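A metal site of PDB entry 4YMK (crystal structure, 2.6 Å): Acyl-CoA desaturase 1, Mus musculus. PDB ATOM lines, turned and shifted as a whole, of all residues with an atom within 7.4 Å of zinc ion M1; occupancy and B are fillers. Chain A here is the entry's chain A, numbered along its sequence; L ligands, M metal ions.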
ATOM      1  N   ASP A  27       5.323  -7.206  29.115  1.00  0.00           N
ATOM      2  CA  ASP A  27       4.017  -7.215  28.458  1.00  0.00           C
ATOM      3  C   ASP A  27       3.476  -5.810  28.285  1.00  0.00           C
ATOM      4  O   ASP A  27       2.320  -5.614  27.883  1.00  0.00           O
ATOM      5  CB  ASP A  27       3.019  -8.070  29.267  1.00  0.00           C
ATOM      6  CG  ASP A  27       2.785  -7.519  30.660  1.00  0.00           C
ATOM      7  OD1 ASP A  27       3.658  -6.800  31.182  1.00  0.00           O
ATOM      8  OD2 ASP A  27       1.711  -7.807  31.230  1.00  0.00           O
ATOM      9  N   HIS A  94      -2.386 -17.440  30.932  1.00  0.00           N
ATOM     10  CA  HIS A  94      -2.607 -16.028  30.639  1.00  0.00           C
ATOM     11  C   HIS A  94      -2.300 -15.134  31.835  1.00  0.00           C
ATOM     12  O   HIS A  94      -1.251 -14.483  31.872  1.00  0.00           O
ATOM     13  CB  HIS A  94      -4.051 -15.816  30.190  1.00  0.00           C
ATOM     14  CG  HIS A  94      -4.325 -14.445  29.661  1.00  0.00           C
ATOM     15  ND1 HIS A  94      -5.354 -13.650  30.133  1.00  0.00           N
ATOM     16  CD2 HIS A  94      -3.697 -13.716  28.708  1.00  0.00           C
ATOM     17  CE1 HIS A  94      -5.348 -12.496  29.486  1.00  0.00           C
ATOM     18  NE2 HIS A  94      -4.351 -12.510  28.623  1.00  0.00           N
ATOM     19  N   ARG A  95      -3.204 -15.096  32.797  1.00  0.00           N
ATOM     20  CA  ARG A  95      -3.121 -14.144  33.898  1.00  0.00           C
ATOM     21  C   ARG A  95      -2.003 -14.435  34.894  1.00  0.00           C
ATOM     22  O   ARG A  95      -1.487 -13.519  35.540  1.00  0.00           O
ATOM     23  CB  ARG A  95      -4.456 -14.085  34.642  1.00  0.00           C
ATOM     24  CG  ARG A  95      -5.629 -13.679  33.748  1.00  0.00           C
ATOM     25  CD  ARG A  95      -6.921 -13.655  34.532  1.00  0.00           C
ATOM     26  NE  ARG A  95      -8.080 -13.415  33.681  1.00  0.00           N
ATOM     27  CZ  ARG A  95      -9.300 -13.161  34.143  1.00  0.00           C
ATOM     28  NH1 ARG A  95      -9.523 -13.115  35.444  1.00  0.00           N
ATOM     29  NH2 ARG A  95     -10.309 -12.957  33.301  1.00  0.00           N
ATOM     30  N   SER A  98       1.904 -15.505  32.067  1.00  0.00           N
ATOM     31  CA  SER A  98       2.245 -14.505  31.057  1.00  0.00           C
ATOM     32  C   SER A  98       2.353 -13.106  31.634  1.00  0.00           C
ATOM     33  O   SER A  98       3.212 -12.326  31.237  1.00  0.00           O
ATOM     34  CB  SER A  98       1.218 -14.508  29.915  1.00  0.00           C
ATOM     35  OG  SER A  98       1.195 -15.748  29.233  1.00  0.00           O
ATOM     36  N   HIS A  99       1.473 -12.790  32.582  1.00  0.00           N
ATOM     37  CA  HIS A  99       1.355 -11.424  33.084  1.00  0.00           C
ATOM     38  C   HIS A  99       1.746 -11.248  34.559  1.00  0.00           C
ATOM     39  O   HIS A  99       1.941 -10.120  35.009  1.00  0.00           O
ATOM     40  CB  HIS A  99      -0.083 -10.930  32.892  1.00  0.00           C
ATOM     41  CG  HIS A  99      -0.485 -10.762  31.456  1.00  0.00           C
ATOM     42  ND1 HIS A  99       0.126  -9.858  30.613  1.00  0.00           N
ATOM     43  CD2 HIS A  99      -1.443 -11.366  30.724  1.00  0.00           C
ATOM     44  CE1 HIS A  99      -0.438  -9.926  29.420  1.00  0.00           C
ATOM     45  NE2 HIS A  99      -1.392 -10.838  29.461  1.00  0.00           N
ATOM     46  N   TRP A 127       3.670 -20.530  25.079  1.00  0.00           N
ATOM     47  CA  TRP A 127       2.433 -19.758  25.060  1.00  0.00           C
ATOM     48  C   TRP A 127       2.687 -18.330  25.544  1.00  0.00           C
ATOM     49  O   TRP A 127       2.245 -17.370  24.920  1.00  0.00           O
ATOM     50  CB  TRP A 127       1.378 -20.426  25.929  1.00  0.00           C
ATOM     51  CG  TRP A 127      -0.036 -19.990  25.650  1.00  0.00           C
ATOM     52  CD1 TRP A 127      -0.964 -20.652  24.913  1.00  0.00           C
ATOM     53  CD2 TRP A 127      -0.675 -18.801  26.129  1.00  0.00           C
ATOM     54  NE1 TRP A 127      -2.143 -19.950  24.885  1.00  0.00           N
ATOM     55  CE2 TRP A 127      -1.999 -18.806  25.632  1.00  0.00           C
ATOM     56  CE3 TRP A 127      -0.270 -17.726  26.927  1.00  0.00           C
ATOM     57  CZ2 TRP A 127      -2.901 -17.784  25.895  1.00  0.00           C
ATOM     58  CZ3 TRP A 127      -1.176 -16.714  27.189  1.00  0.00           C
ATOM     59  CH2 TRP A 127      -2.478 -16.749  26.676  1.00  0.00           C
ATOM     60  N   HIS A 131       2.763 -14.545  23.748  1.00  0.00           N
ATOM     61  CA  HIS A 131       1.774 -13.619  24.279  1.00  0.00           C
ATOM     62  C   HIS A 131       2.389 -12.298  24.722  1.00  0.00           C
ATOM     63  O   HIS A 131       1.815 -11.238  24.500  1.00  0.00           O
ATOM     64  CB  HIS A 131       1.008 -14.249  25.429  1.00  0.00           C
ATOM     65  CG  HIS A 131      -0.193 -13.458  25.846  1.00  0.00           C
ATOM     66  ND1 HIS A 131      -1.243 -13.201  24.997  1.00  0.00           N
ATOM     67  CD2 HIS A 131      -0.485 -12.837  27.014  1.00  0.00           C
ATOM     68  CE1 HIS A 131      -2.142 -12.470  25.626  1.00  0.00           C
ATOM     69  NE2 HIS A 131      -1.717 -12.231  26.853  1.00  0.00           N
ATOM     70  N   ARG A 132       3.554 -12.378  25.361  1.00  0.00           N
ATOM     71  CA  ARG A 132       4.263 -11.162  25.761  1.00  0.00           C
ATOM     72  C   ARG A 132       4.649 -10.349  24.525  1.00  0.00           C
ATOM     73  O   ARG A 132       4.588  -9.129  24.548  1.00  0.00           O
ATOM     74  CB  ARG A 132       5.492 -11.522  26.595  1.00  0.00           C
ATOM     75  CG  ARG A 132       5.143 -12.088  27.961  1.00  0.00           C
ATOM     76  CD  ARG A 132       6.358 -12.515  28.761  1.00  0.00           C
ATOM     77  NE  ARG A 132       5.968 -13.024  30.069  1.00  0.00           N
ATOM     78  CZ  ARG A 132       6.821 -13.450  30.991  1.00  0.00           C
ATOM     79  NH1 ARG A 132       8.134 -13.438  30.762  1.00  0.00           N
ATOM     80  NH2 ARG A 132       6.364 -13.903  32.153  1.00  0.00           N
ATOM     81  N   HIS A 134       2.949 -10.467  21.822  1.00  0.00           N
ATOM     82  CA  HIS A 134       1.650 -10.020  21.331  1.00  0.00           C
ATOM     83  C   HIS A 134       1.209  -8.719  21.993  1.00  0.00           C
ATOM     84  O   HIS A 134       0.478  -7.926  21.402  1.00  0.00           O
ATOM     85  CB  HIS A 134       0.591 -11.100  21.555  1.00  0.00           C
ATOM     86  CG  HIS A 134      -0.812 -10.632  21.350  1.00  0.00           C
ATOM     87  ND1 HIS A 134      -1.324 -10.332  20.107  1.00  0.00           N
ATOM     88  CD2 HIS A 134      -1.817 -10.417  22.232  1.00  0.00           C
ATOM     89  CE1 HIS A 134      -2.579  -9.940  20.226  1.00  0.00           C
ATOM     90  NE2 HIS A 134      -2.906  -9.978  21.507  1.00  0.00           N
ATOM     91  N   HIS A 135       1.671  -8.496  23.227  1.00  0.00           N
ATOM     92  CA  HIS A 135       1.311  -7.296  23.975  1.00  0.00           C
ATOM     93  C   HIS A 135       2.287  -6.142  23.725  1.00  0.00           C
ATOM     94  O   HIS A 135       1.869  -5.011  23.513  1.00  0.00           O
ATOM     95  CB  HIS A 135       1.254  -7.600  25.472  1.00  0.00           C
ATOM     96  CG  HIS A 135      -0.081  -8.101  25.939  1.00  0.00           C
ATOM     97  ND1 HIS A 135      -1.043  -7.264  26.455  1.00  0.00           N
ATOM     98  CD2 HIS A 135      -0.595  -9.347  25.965  1.00  0.00           C
ATOM     99  CE1 HIS A 135      -2.110  -7.973  26.770  1.00  0.00           C
ATOM    100  NE2 HIS A 135      -1.865  -9.242  26.488  1.00  0.00           N
ATOM    101  N   GLU A 269     -12.342 -13.434  29.011  1.00  0.00           N
ATOM    102  CA  GLU A 269     -11.225 -12.809  28.297  1.00  0.00           C
ATOM    103  C   GLU A 269     -11.694 -12.002  27.096  1.00  0.00           C
ATOM    104  O   GLU A 269     -10.940 -11.838  26.125  1.00  0.00           O
ATOM    105  CB  GLU A 269     -10.218 -13.873  27.851  1.00  0.00           C
ATOM    106  CG  GLU A 269      -9.785 -14.828  28.933  1.00  0.00           C
ATOM    107  CD  GLU A 269      -9.150 -14.141  30.132  1.00  0.00           C
ATOM    108  OE1 GLU A 269      -7.920 -13.991  30.142  1.00  0.00           O
ATOM    109  OE2 GLU A 269      -9.892 -13.777  31.066  1.00  0.00           O
ATOM    110  N   HIS A 272     -11.108  -7.109  26.047  1.00  0.00           N
ATOM    111  CA  HIS A 272      -9.757  -7.065  25.530  1.00  0.00           C
ATOM    112  C   HIS A 272      -9.194  -5.647  25.444  1.00  0.00           C
ATOM    113  O   HIS A 272      -7.973  -5.453  25.493  1.00  0.00           O
ATOM    114  CB  HIS A 272      -9.710  -7.718  24.151  1.00  0.00           C
ATOM    115  CG  HIS A 272      -8.411  -8.400  23.846  1.00  0.00           C
ATOM    116  ND1 HIS A 272      -7.731  -9.157  24.783  1.00  0.00           N
ATOM    117  CD2 HIS A 272      -7.666  -8.437  22.719  1.00  0.00           C
ATOM    118  CE1 HIS A 272      -6.622  -9.628  24.237  1.00  0.00           C
ATOM    119  NE2 HIS A 272      -6.557  -9.207  22.987  1.00  0.00           N
ATOM    120  N   HIS A 275      -7.900  -5.059  28.894  1.00  0.00           N
ATOM    121  CA  HIS A 275      -6.756  -5.922  29.159  1.00  0.00           C
ATOM    122  C   HIS A 275      -5.471  -5.437  28.508  1.00  0.00           C
ATOM    123  O   HIS A 275      -4.412  -5.443  29.126  1.00  0.00           O
ATOM    124  CB  HIS A 275      -7.050  -7.357  28.697  1.00  0.00           C
ATOM    125  CG  HIS A 275      -5.880  -8.273  28.814  1.00  0.00           C
ATOM    126  ND1 HIS A 275      -5.279  -8.544  30.023  1.00  0.00           N
ATOM    127  CD2 HIS A 275      -5.181  -8.960  27.880  1.00  0.00           C
ATOM    128  CE1 HIS A 275      -4.268  -9.380  29.834  1.00  0.00           C
ATOM    129  NE2 HIS A 275      -4.182  -9.638  28.535  1.00  0.00           N
ATOM    130  N   HIS A 276      -5.555  -5.001  27.249  1.00  0.00           N
ATOM    131  CA  HIS A 276      -4.371  -4.487  26.558  1.00  0.00           C
ATOM    132  C   HIS A 276      -3.927  -3.156  27.151  1.00  0.00           C
ATOM    133  O   HIS A 276      -2.752  -2.798  27.090  1.00  0.00           O
ATOM    134  CB  HIS A 276      -4.629  -4.347  25.060  1.00  0.00           C
ATOM    135  CG  HIS A 276      -4.223  -5.542  24.259  1.00  0.00           C
ATOM    136  ND1 HIS A 276      -2.940  -5.713  23.790  1.00  0.00           N
ATOM    137  CD2 HIS A 276      -4.918  -6.632  23.873  1.00  0.00           C
ATOM    138  CE1 HIS A 276      -2.872  -6.853  23.126  1.00  0.00           C
ATOM    139  NE2 HIS A 276      -4.055  -7.426  23.154  1.00  0.00           N
ATOM    140  N   PRO A 279      -2.543  -4.632  31.284  1.00  0.00           N
ATOM    141  CA  PRO A 279      -2.183  -6.055  31.249  1.00  0.00           C
ATOM    142  C   PRO A 279      -1.775  -6.617  32.612  1.00  0.00           C
ATOM    143  O   PRO A 279      -1.634  -7.835  32.758  1.00  0.00           O
ATOM    144  CB  PRO A 279      -1.007  -6.096  30.269  1.00  0.00           C
ATOM    145  CG  PRO A 279      -0.408  -4.744  30.352  1.00  0.00           C
ATOM    146  CD  PRO A 279      -1.542  -3.800  30.579  1.00  0.00           C
ATOM    147  N   ALA A 284      -8.467  -8.793  34.395  1.00  0.00           N
ATOM    148  CA  ALA A 284      -8.497  -8.531  32.953  1.00  0.00           C
ATOM    149  C   ALA A 284      -9.779  -7.801  32.548  1.00  0.00           C
ATOM    150  O   ALA A 284     -10.219  -7.897  31.400  1.00  0.00           O
ATOM    151  CB  ALA A 284      -8.348  -9.830  32.172  1.00  0.00           C
HETATM  152  C1  LIG L   1      -2.740 -22.537  19.884  1.00  0.00           C
HETATM  153  C2  LIG L   1      -2.434 -21.446  20.876  1.00  0.00           C
HETATM  154  O1  LIG L   1      -3.775 -22.530  19.260  1.00  0.00           O
HETATM  155  C3  LIG L   1      -2.852 -20.083  20.319  1.00  0.00           C
HETATM  156  C4  LIG L   1      -3.959 -19.477  21.182  1.00  0.00           C
HETATM  157  C5  LIG L   1      -3.348 -18.567  22.245  1.00  0.00           C
HETATM  158  C6  LIG L   1      -3.604 -17.102  21.914  1.00  0.00           C
HETATM  159  C7  LIG L   1      -4.552 -16.474  22.941  1.00  0.00           C
HETATM  160  C8  LIG L   1      -4.045 -15.076  23.322  1.00  0.00           C
HETATM  161  C9  LIG L   1      -5.234 -14.137  23.528  1.00  0.00           C
HETATM  162  C10 LIG L   1      -5.283 -13.644  24.978  1.00  0.00           C
HETATM  163  C11 LIG L   1      -5.645 -14.784  25.921  1.00  0.00           C
HETATM  164  C12 LIG L   1      -7.076 -15.269  25.656  1.00  0.00           C
HETATM  165  C13 LIG L   1      -7.318 -16.589  26.408  1.00  0.00           C
HETATM  166  C14 LIG L   1      -8.717 -17.128  26.078  1.00  0.00           C
HETATM  167  C15 LIG L   1      -8.842 -18.566  26.578  1.00  0.00           C
HETATM  168  C16 LIG L   1     -10.247 -19.096  26.297  1.00  0.00           C
HETATM  169  C17 LIG L   1     -10.353 -20.560  26.750  1.00  0.00           C
HETATM  170  C18 LIG L   1     -11.752 -21.090  26.440  1.00  0.00           C
HETATM  171  N1  LIG L   1       9.656 -15.188  20.761  1.00  0.00           N
HETATM  172  O2  LIG L   1       7.361 -21.925  16.376  1.00  0.00           O
HETATM  173  P1  LIG L   1       8.603 -22.013  15.572  1.00  0.00           P
HETATM  174  C19 LIG L   1      11.935 -18.806  17.866  1.00  0.00           C
HETATM  175  S1  LIG L   1      -1.602 -23.803  19.657  1.00  0.00           S
HETATM  176  C20 LIG L   1      10.941 -15.471  20.638  1.00  0.00           C
HETATM  177  O3  LIG L   1       8.899 -23.536  15.156  1.00  0.00           O
HETATM  178  P2  LIG L   1       8.033 -21.456  12.729  1.00  0.00           P
HETATM  179  C21 LIG L   1      12.501 -19.727  18.985  1.00  0.00           C
HETATM  180  O4  LIG L   1      13.919 -19.676  19.001  1.00  0.00           O
HETATM  181  C22 LIG L   1      -2.693 -25.140  19.129  1.00  0.00           C
HETATM  182  N2  LIG L   1      11.379 -16.428  19.855  1.00  0.00           N
HETATM  183  O5  LIG L   1       8.439 -21.114  14.248  1.00  0.00           O
HETATM  184  C23 LIG L   1      12.007 -21.125  18.535  1.00  0.00           C
HETATM  185  O6  LIG L   1      12.856 -22.152  19.046  1.00  0.00           O
HETATM  186  P3  LIG L   1      12.412 -23.154  20.229  1.00  0.00           P
HETATM  187  C24 LIG L   1      -1.886 -26.450  19.101  1.00  0.00           C
HETATM  188  C25 LIG L   1      10.524 -17.160  19.152  1.00  0.00           C
HETATM  189  O7  LIG L   1       9.076 -22.511  12.126  1.00  0.00           O
HETATM  190  C26 LIG L   1      12.129 -21.003  17.010  1.00  0.00           C
HETATM  191  O8  LIG L   1      11.763 -19.643  16.697  1.00  0.00           O
HETATM  192  N3  LIG L   1      -0.495 -26.140  18.746  1.00  0.00           N
HETATM  193  C27 LIG L   1       9.147 -16.910  19.257  1.00  0.00           C
HETATM  194  O9  LIG L   1       8.026 -20.205  11.926  1.00  0.00           O
HETATM  195  C28 LIG L   1      11.161 -21.961  16.325  1.00  0.00           C
HETATM  196  O10 LIG L   1       9.837 -21.438  16.431  1.00  0.00           O
HETATM  197  C29 LIG L   1      -0.142 -26.080  17.440  1.00  0.00           C
HETATM  198  O11 LIG L   1      -0.959 -26.283  16.574  1.00  0.00           O
HETATM  199  C30 LIG L   1       8.726 -15.868  20.105  1.00  0.00           C
HETATM  200  N4  LIG L   1       7.388 -15.564  20.258  1.00  0.00           N
HETATM  201  O12 LIG L   1       6.552 -22.099  12.728  1.00  0.00           O
HETATM  202  C31 LIG L   1       1.287 -25.752  17.052  1.00  0.00           C
HETATM  203  N5  LIG L   1       8.517 -17.803  18.445  1.00  0.00           N
HETATM  204  O13 LIG L   1      11.295 -22.450  21.152  1.00  0.00           O
HETATM  205  C32 LIG L   1       1.256 -25.119  15.662  1.00  0.00           C
HETATM  206  C33 LIG L   1       9.405 -18.556  17.875  1.00  0.00           C
HETATM  207  O14 LIG L   1      11.787 -24.484  19.580  1.00  0.00           O
HETATM  208  N6  LIG L   1       2.299 -24.083  15.526  1.00  0.00           N
HETATM  209  N7  LIG L   1      10.662 -18.214  18.279  1.00  0.00           N
HETATM  210  O15 LIG L   1      13.594 -23.501  21.044  1.00  0.00           O
HETATM  211  C34 LIG L   1       3.414 -24.353  14.809  1.00  0.00           C
HETATM  212  O16 LIG L   1       3.530 -25.443  14.308  1.00  0.00           O
HETATM  213  C35 LIG L   1       4.500 -23.313  14.641  1.00  0.00           C
HETATM  214  O17 LIG L   1       4.570 -22.496  15.820  1.00  0.00           O
HETATM  215  C36 LIG L   1       4.266 -22.425  13.415  1.00  0.00           C
HETATM  216  C37 LIG L   1       5.428 -21.436  13.302  1.00  0.00           C
HETATM  217  C38 LIG L   1       2.959 -21.646  13.545  1.00  0.00           C
HETATM  218  C39 LIG L   1       4.232 -23.272  12.151  1.00  0.00           C
HETATM  219 ZN    ZN M   1      -2.790 -10.828  27.777  1.00  0.00          ZN
HETATM  220 ZN    ZN M   2      -4.872  -9.169  21.966  1.00  0.00          ZN
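A ring nitrogen (ND1) of His 99 sits close to the backbone carbonyl oxygen of Pro 279 (3.4 Å). The side-chain carboxylate of Asp 27 is in hydrogen-bond range of a ring nitrogen (ND1) of His 99, 2.7 Å away. ND1 of His 94 is in hydrogen-bond range of OE1 of Glu 269, at 2.6 Å.
The nearest printed residue that does not touch zinc ion M1 is His 272 (5.4 Å).
Zinc ion M1 is bound by a ring nitrogen (NE2) of His 275 (2.0 Å), a ring nitrogen (NE2) of His 131 (2.0 Å), a ring nitrogen (NE2) of His 99 (2.2 Å), a ring nitrogen (NE2) of His 135 (2.2 Å) and a ring nitrogen (NE2) of His 94 (2.4 Å).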
